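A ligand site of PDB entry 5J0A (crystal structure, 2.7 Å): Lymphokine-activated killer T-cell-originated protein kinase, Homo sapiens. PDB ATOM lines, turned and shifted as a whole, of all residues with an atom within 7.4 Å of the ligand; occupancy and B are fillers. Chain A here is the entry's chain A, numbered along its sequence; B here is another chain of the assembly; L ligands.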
ATOM      1  N   VAL A  56      20.909   6.279 -32.971  1.00  0.00           N
ATOM      2  CA  VAL A  56      20.727   7.090 -31.766  1.00  0.00           C
ATOM      3  C   VAL A  56      20.534   8.567 -32.107  1.00  0.00           C
ATOM      4  O   VAL A  56      19.528   9.177 -31.740  1.00  0.00           O
ATOM      5  CB  VAL A  56      21.936   6.934 -30.789  1.00  0.00           C
ATOM      6  CG1 VAL A  56      21.819   7.893 -29.651  1.00  0.00           C
ATOM      7  CG2 VAL A  56      21.984   5.501 -30.269  1.00  0.00           C
ATOM      8  N   TYR A  57      21.495   9.136 -32.835  1.00  0.00           N
ATOM      9  CA  TYR A  57      21.459  10.547 -33.227  1.00  0.00           C
ATOM     10  C   TYR A  57      20.889  10.697 -34.628  1.00  0.00           C
ATOM     11  O   TYR A  57      21.619  10.800 -35.618  1.00  0.00           O
ATOM     12  CB  TYR A  57      22.873  11.133 -33.107  1.00  0.00           C
ATOM     13  CG  TYR A  57      23.375  10.984 -31.689  1.00  0.00           C
ATOM     14  CD1 TYR A  57      22.862  11.779 -30.672  1.00  0.00           C
ATOM     15  CD2 TYR A  57      24.240   9.947 -31.337  1.00  0.00           C
ATOM     16  CE1 TYR A  57      23.181  11.545 -29.342  1.00  0.00           C
ATOM     17  CE2 TYR A  57      24.561   9.703 -30.010  1.00  0.00           C
ATOM     18  CZ  TYR A  57      24.029  10.503 -29.016  1.00  0.00           C
ATOM     19  OH  TYR A  57      24.301  10.248 -27.690  1.00  0.00           O
ATOM     20  N   VAL A  77       8.087  10.441 -23.270  1.00  0.00           N
ATOM     21  CA  VAL A  77       9.536  10.502 -23.329  1.00  0.00           C
ATOM     22  C   VAL A  77       9.795  11.401 -24.517  1.00  0.00           C
ATOM     23  O   VAL A  77       9.323  11.130 -25.632  1.00  0.00           O
ATOM     24  CB  VAL A  77      10.168   9.100 -23.574  1.00  0.00           C
ATOM     25  CG1 VAL A  77      11.674   9.222 -23.642  1.00  0.00           C
ATOM     26  CG2 VAL A  77       9.797   8.160 -22.458  1.00  0.00           C
ATOM     27  N   GLY A  78      10.515  12.492 -24.295  1.00  0.00           N
ATOM     28  CA  GLY A  78      10.788  13.418 -25.372  1.00  0.00           C
ATOM     29  C   GLY A  78      12.171  13.254 -25.981  1.00  0.00           C
ATOM     30  O   GLY A  78      12.806  12.205 -25.822  1.00  0.00           O
ATOM     31  N   ARG A  80      16.033  15.438 -27.328  1.00  0.00           N
ATOM     32  CA  ARG A  80      16.942  16.534 -27.064  1.00  0.00           C
ATOM     33  C   ARG A  80      17.944  16.649 -28.186  1.00  0.00           C
ATOM     34  O   ARG A  80      18.314  15.653 -28.806  1.00  0.00           O
ATOM     35  CB  ARG A  80      17.686  16.335 -25.750  1.00  0.00           C
ATOM     36  CG  ARG A  80      18.696  15.212 -25.784  1.00  0.00           C
ATOM     37  CD  ARG A  80      19.726  15.376 -24.691  1.00  0.00           C
ATOM     38  NE  ARG A  80      19.121  15.383 -23.365  1.00  0.00           N
ATOM     39  CZ  ARG A  80      19.823  15.528 -22.240  1.00  0.00           C
ATOM     40  NH1 ARG A  80      21.135  15.664 -22.290  1.00  0.00           N
ATOM     41  NH2 ARG A  80      19.199  15.534 -21.068  1.00  0.00           N
ATOM     42  N   PHE A  82      21.758  18.604 -29.679  1.00  0.00           N
ATOM     43  CA  PHE A  82      23.077  18.929 -29.175  1.00  0.00           C
ATOM     44  C   PHE A  82      23.781  20.100 -29.829  1.00  0.00           C
ATOM     45  O   PHE A  82      24.967  20.330 -29.588  1.00  0.00           O
ATOM     46  CB  PHE A  82      23.943  17.672 -29.259  1.00  0.00           C
ATOM     47  CG  PHE A  82      23.271  16.448 -28.707  1.00  0.00           C
ATOM     48  CD1 PHE A  82      22.381  15.724 -29.494  1.00  0.00           C
ATOM     49  CD2 PHE A  82      23.464  16.056 -27.380  1.00  0.00           C
ATOM     50  CE1 PHE A  82      21.688  14.644 -28.964  1.00  0.00           C
ATOM     51  CE2 PHE A  82      22.777  14.990 -26.851  1.00  0.00           C
ATOM     52  CZ  PHE A  82      21.887  14.280 -27.649  1.00  0.00           C
ATOM     53  N   ALA A  93      17.985  12.913 -30.167  1.00  0.00           N
ATOM     54  CA  ALA A  93      18.110  11.639 -29.471  1.00  0.00           C
ATOM     55  C   ALA A  93      16.963  11.538 -28.502  1.00  0.00           C
ATOM     56  O   ALA A  93      16.629  12.501 -27.800  1.00  0.00           O
ATOM     57  CB  ALA A  93      19.439  11.555 -28.737  1.00  0.00           C
ATOM     58  N   MET A  94      16.328  10.377 -28.454  1.00  0.00           N
ATOM     59  CA  MET A  94      15.236  10.166 -27.538  1.00  0.00           C
ATOM     60  C   MET A  94      15.824  10.158 -26.126  1.00  0.00           C
ATOM     61  O   MET A  94      16.883   9.587 -25.887  1.00  0.00           O
ATOM     62  CB  MET A  94      14.554   8.849 -27.861  1.00  0.00           C
ATOM     63  CG  MET A  94      13.334   8.536 -27.041  1.00  0.00           C
ATOM     64  SD  MET A  94      12.403   7.258 -27.858  1.00  0.00           S
ATOM     65  CE  MET A  94      13.525   5.915 -27.761  1.00  0.00           C
ATOM     66  N   GLU A  95      15.158  10.804 -25.181  1.00  0.00           N
ATOM     67  CA  GLU A  95      15.639  10.833 -23.817  1.00  0.00           C
ATOM     68  C   GLU A  95      15.331   9.562 -23.037  1.00  0.00           C
ATOM     69  O   GLU A  95      14.583   8.710 -23.481  1.00  0.00           O
ATOM     70  CB  GLU A  95      15.119  12.092 -23.116  1.00  0.00           C
ATOM     71  CG  GLU A  95      15.659  13.353 -23.787  1.00  0.00           C
ATOM     72  CD  GLU A  95      15.555  14.598 -22.947  1.00  0.00           C
ATOM     73  OE1 GLU A  95      16.396  15.503 -23.121  1.00  0.00           O
ATOM     74  OE2 GLU A  95      14.637  14.673 -22.110  1.00  0.00           O
ATOM     75  N   TYR A  96      15.936   9.446 -21.855  1.00  0.00           N
ATOM     76  CA  TYR A  96      15.787   8.283 -21.004  1.00  0.00           C
ATOM     77  C   TYR A  96      14.560   8.348 -20.122  1.00  0.00           C
ATOM     78  O   TYR A  96      14.179   9.432 -19.659  1.00  0.00           O
ATOM     79  CB  TYR A  96      17.054   8.140 -20.177  1.00  0.00           C
ATOM     80  CG  TYR A  96      17.042   7.125 -19.057  1.00  0.00           C
ATOM     81  CD1 TYR A  96      16.618   7.484 -17.776  1.00  0.00           C
ATOM     82  CD2 TYR A  96      17.507   5.824 -19.262  1.00  0.00           C
ATOM     83  CE1 TYR A  96      16.694   6.583 -16.734  1.00  0.00           C
ATOM     84  CE2 TYR A  96      17.578   4.915 -18.231  1.00  0.00           C
ATOM     85  CZ  TYR A  96      17.173   5.303 -16.960  1.00  0.00           C
ATOM     86  OH  TYR A  96      17.290   4.409 -15.911  1.00  0.00           O
ATOM     87  N   GLY A  97      13.933   7.199 -19.894  1.00  0.00           N
ATOM     88  CA  GLY A  97      12.751   7.160 -19.056  1.00  0.00           C
ATOM     89  C   GLY A  97      12.682   5.896 -18.237  1.00  0.00           C
ATOM     90  O   GLY A  97      11.586   5.446 -17.886  1.00  0.00           O
ATOM     91  N   VAL B  60      18.956   2.937 -28.423  1.00  0.00           N
ATOM     92  CA  VAL B  60      19.820   3.919 -27.789  1.00  0.00           C
ATOM     93  C   VAL B  60      20.179   3.554 -26.346  1.00  0.00           C
ATOM     94  O   VAL B  60      21.317   3.700 -25.935  1.00  0.00           O
ATOM     95  CB  VAL B  60      19.190   5.363 -27.893  1.00  0.00           C
ATOM     96  CG1 VAL B  60      17.816   5.273 -28.478  1.00  0.00           C
ATOM     97  CG2 VAL B  60      19.157   6.057 -26.545  1.00  0.00           C
ATOM     98  N   TYR B  61      19.209   3.057 -25.583  1.00  0.00           N
ATOM     99  CA  TYR B  61      19.474   2.674 -24.208  1.00  0.00           C
ATOM    100  C   TYR B  61      19.609   1.164 -24.166  1.00  0.00           C
ATOM    101  O   TYR B  61      18.634   0.436 -24.020  1.00  0.00           O
ATOM    102  CB  TYR B  61      18.341   3.154 -23.301  1.00  0.00           C
ATOM    103  CG  TYR B  61      18.223   4.655 -23.307  1.00  0.00           C
ATOM    104  CD1 TYR B  61      19.148   5.453 -22.640  1.00  0.00           C
ATOM    105  CD2 TYR B  61      17.235   5.295 -24.076  1.00  0.00           C
ATOM    106  CE1 TYR B  61      19.104   6.847 -22.726  1.00  0.00           C
ATOM    107  CE2 TYR B  61      17.187   6.681 -24.173  1.00  0.00           C
ATOM    108  CZ  TYR B  61      18.124   7.451 -23.508  1.00  0.00           C
ATOM    109  OH  TYR B  61      18.103   8.830 -23.629  1.00  0.00           O
ATOM    110  N   ARG B  84      27.263   6.541 -21.518  1.00  0.00           N
ATOM    111  CA  ARG B  84      26.671   7.225 -20.392  1.00  0.00           C
ATOM    112  C   ARG B  84      25.594   6.362 -19.766  1.00  0.00           C
ATOM    113  O   ARG B  84      24.796   5.746 -20.465  1.00  0.00           O
ATOM    114  CB  ARG B  84      26.076   8.533 -20.904  1.00  0.00           C
ATOM    115  CG  ARG B  84      25.309   9.361 -19.920  1.00  0.00           C
ATOM    116  CD  ARG B  84      25.094  10.722 -20.552  1.00  0.00           C
ATOM    117  NE  ARG B  84      24.185  11.590 -19.824  1.00  0.00           N
ATOM    118  CZ  ARG B  84      24.112  12.902 -20.059  1.00  0.00           C
ATOM    119  NH1 ARG B  84      24.883  13.449 -20.988  1.00  0.00           N
ATOM    120  NH2 ARG B  84      23.251  13.657 -19.378  1.00  0.00           N
ATOM    121  N   PHE B  86      22.428   5.996 -16.759  1.00  0.00           N
ATOM    122  CA  PHE B  86      21.401   6.903 -16.293  1.00  0.00           C
ATOM    123  C   PHE B  86      20.817   6.548 -14.946  1.00  0.00           C
ATOM    124  O   PHE B  86      19.789   7.087 -14.547  1.00  0.00           O
ATOM    125  CB  PHE B  86      20.301   7.006 -17.357  1.00  0.00           C
ATOM    126  CG  PHE B  86      20.790   7.541 -18.658  1.00  0.00           C
ATOM    127  CD1 PHE B  86      21.449   6.725 -19.563  1.00  0.00           C
ATOM    128  CD2 PHE B  86      20.669   8.895 -18.949  1.00  0.00           C
ATOM    129  CE1 PHE B  86      21.988   7.250 -20.749  1.00  0.00           C
ATOM    130  CE2 PHE B  86      21.205   9.429 -20.133  1.00  0.00           C
ATOM    131  CZ  PHE B  86      21.870   8.612 -21.030  1.00  0.00           C
ATOM    132  N   ALA B  97      23.937   4.444 -23.036  1.00  0.00           N
ATOM    133  CA  ALA B  97      23.673   5.063 -24.341  1.00  0.00           C
ATOM    134  C   ALA B  97      24.998   5.605 -24.864  1.00  0.00           C
ATOM    135  O   ALA B  97      25.760   6.201 -24.100  1.00  0.00           O
ATOM    136  CB  ALA B  97      22.669   6.184 -24.209  1.00  0.00           C
ATOM    137  N   MET B  98      25.282   5.390 -26.148  1.00  0.00           N
ATOM    138  CA  MET B  98      26.515   5.892 -26.733  1.00  0.00           C
ATOM    139  C   MET B  98      26.450   7.410 -26.727  1.00  0.00           C
ATOM    140  O   MET B  98      25.427   8.016 -27.040  1.00  0.00           O
ATOM    141  CB  MET B  98      26.677   5.364 -28.157  1.00  0.00           C
ATOM    142  CG  MET B  98      27.787   6.033 -28.977  1.00  0.00           C
ATOM    143  SD  MET B  98      28.290   4.994 -30.371  1.00  0.00           S
ATOM    144  CE  MET B  98      26.823   5.069 -31.372  1.00  0.00           C
ATOM    145  N   GLU B  99      27.554   8.048 -26.342  1.00  0.00           N
ATOM    146  CA  GLU B  99      27.611   9.486 -26.280  1.00  0.00           C
ATOM    147  C   GLU B  99      27.631  10.186 -27.636  1.00  0.00           C
ATOM    148  O   GLU B  99      27.781   9.562 -28.687  1.00  0.00           O
ATOM    149  CB  GLU B  99      28.798   9.924 -25.425  1.00  0.00           C
ATOM    150  CG  GLU B  99      28.472   9.954 -23.958  1.00  0.00           C
ATOM    151  CD  GLU B  99      29.676  10.240 -23.091  1.00  0.00           C
ATOM    152  OE1 GLU B  99      29.501  10.778 -21.969  1.00  0.00           O
ATOM    153  OE2 GLU B  99      30.811   9.922 -23.524  1.00  0.00           O
ATOM    154  N   TYR B 100      27.470  11.504 -27.587  1.00  0.00           N
ATOM    155  CA  TYR B 100      27.451  12.354 -28.750  1.00  0.00           C
ATOM    156  C   TYR B 100      28.828  12.896 -29.094  1.00  0.00           C
ATOM    157  O   TYR B 100      29.580  13.319 -28.222  1.00  0.00           O
ATOM    158  CB  TYR B 100      26.477  13.496 -28.508  1.00  0.00           C
ATOM    159  CG  TYR B 100      26.435  14.513 -29.609  1.00  0.00           C
ATOM    160  CD1 TYR B 100      25.762  14.259 -30.803  1.00  0.00           C
ATOM    161  CD2 TYR B 100      27.062  15.749 -29.452  1.00  0.00           C
ATOM    162  CE1 TYR B 100      25.717  15.208 -31.809  1.00  0.00           C
ATOM    163  CE2 TYR B 100      27.030  16.700 -30.456  1.00  0.00           C
ATOM    164  CZ  TYR B 100      26.357  16.427 -31.628  1.00  0.00           C
ATOM    165  OH  TYR B 100      26.349  17.386 -32.610  1.00  0.00           O
ATOM    166  N   GLY B 101      29.155  12.870 -30.391  1.00  0.00           N
ATOM    167  CA  GLY B 101      30.453  13.361 -30.822  1.00  0.00           C
ATOM    168  C   GLY B 101      30.384  14.201 -32.078  1.00  0.00           C
ATOM    169  O   GLY B 101      31.396  14.401 -32.747  1.00  0.00           O
HETATM  170  C1  LIG L   1      18.279  12.196 -20.309  1.00  0.00           C
HETATM  171  O1  LIG L   1      18.344  12.654 -19.151  1.00  0.00           O
HETATM  172  O2  LIG L   1      17.243  11.691 -20.804  1.00  0.00           O
HETATM  173  C2  LIG L   1      19.421  12.252 -21.099  1.00  0.00           C
HETATM  174  C3  LIG L   1      19.475  11.565 -22.305  1.00  0.00           C
HETATM  175  C4  LIG L   1      20.601  11.601 -23.111  1.00  0.00           C
HETATM  176  C5  LIG L   1      20.622  10.883 -24.309  1.00  0.00           C
HETATM  177  C6  LIG L   1      21.753  10.886 -25.112  1.00  0.00           C
HETATM  178  C7  LIG L   1      22.878  11.616 -24.728  1.00  0.00           C
HETATM  179  C8  LIG L   1      22.859  12.325 -23.533  1.00  0.00           C
HETATM  180  C9  LIG L   1      21.728  12.321 -22.730  1.00  0.00           C
HETATM  181  O3  LIG L   1      23.967  11.653 -25.529  1.00  0.00           O
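O3 of the ligand lies within hydrogen-bond range of OH of Tyr 57 (2.6 Å). The guanidinium group (NH2) of Arg 80 is in salt-bridge range of an oxygen (O1) of the ligand (3.6 Å). N of Tyr 96 is in hydrogen-bond range of O2 of the ligand, at 2.8 Å.
The side-chain carboxylate of Glu 95 lies within salt-bridge range of the guanidinium group of Arg 80 (2.7 Å). The backbone carbonyl oxygen (O) of Met 94 is in hydrogen-bond range of the side-chain hydroxyl (OH) of Tyr 61 of chain B. N of Ala 97 of chain B sits at hydrogen-bond distance from O of Arg 84 of chain B, at 3.0 Å. The backbone NH (N) of Arg 80 lies within hydrogen-bond range of the backbone carbonyl oxygen (O) of Ala 93 (3.0 Å). The backbone NH of Glu 95 is in hydrogen-bond range of the backbone carbonyl oxygen of Gly 78 (2.8 Å). The side-chain hydroxyl of Tyr 61 of chain B lies within hydrogen-bond range of the backbone NH of Tyr 96, at 2.9 Å. The side-chain hydroxyl of Tyr 57 sits at hydrogen-bond distance from the backbone carbonyl oxygen of Met 98 of chain B (2.6 Å). The side-chain hydroxyl (OH) of Tyr 57 sits at hydrogen-bond distance from the backbone NH (N) of Tyr 100 of chain B (3.4 Å).
Merely in contact with the ligand: Glu 95 (3.2 Å), Tyr 61 of chain B (3.3 Å), Arg 84 of chain B (3.4 Å), Phe 86 of chain B (3.5 Å) and Phe 82 (3.8 Å). Hydrophobic or aromatic side chains within 4 Å of the ligand: Tyr 57, Phe 82, Tyr 96 and Phe 86 of chain B. Within 4 Å of the ligand: Tyr 57, Arg 80, Phe 82, Glu 95, Tyr 96, Tyr 61 of chain B, Arg 84 of chain B and Phe 86 of chain B. Along chain A the residues within 4 Å of the ligand span positions 57 to 96.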
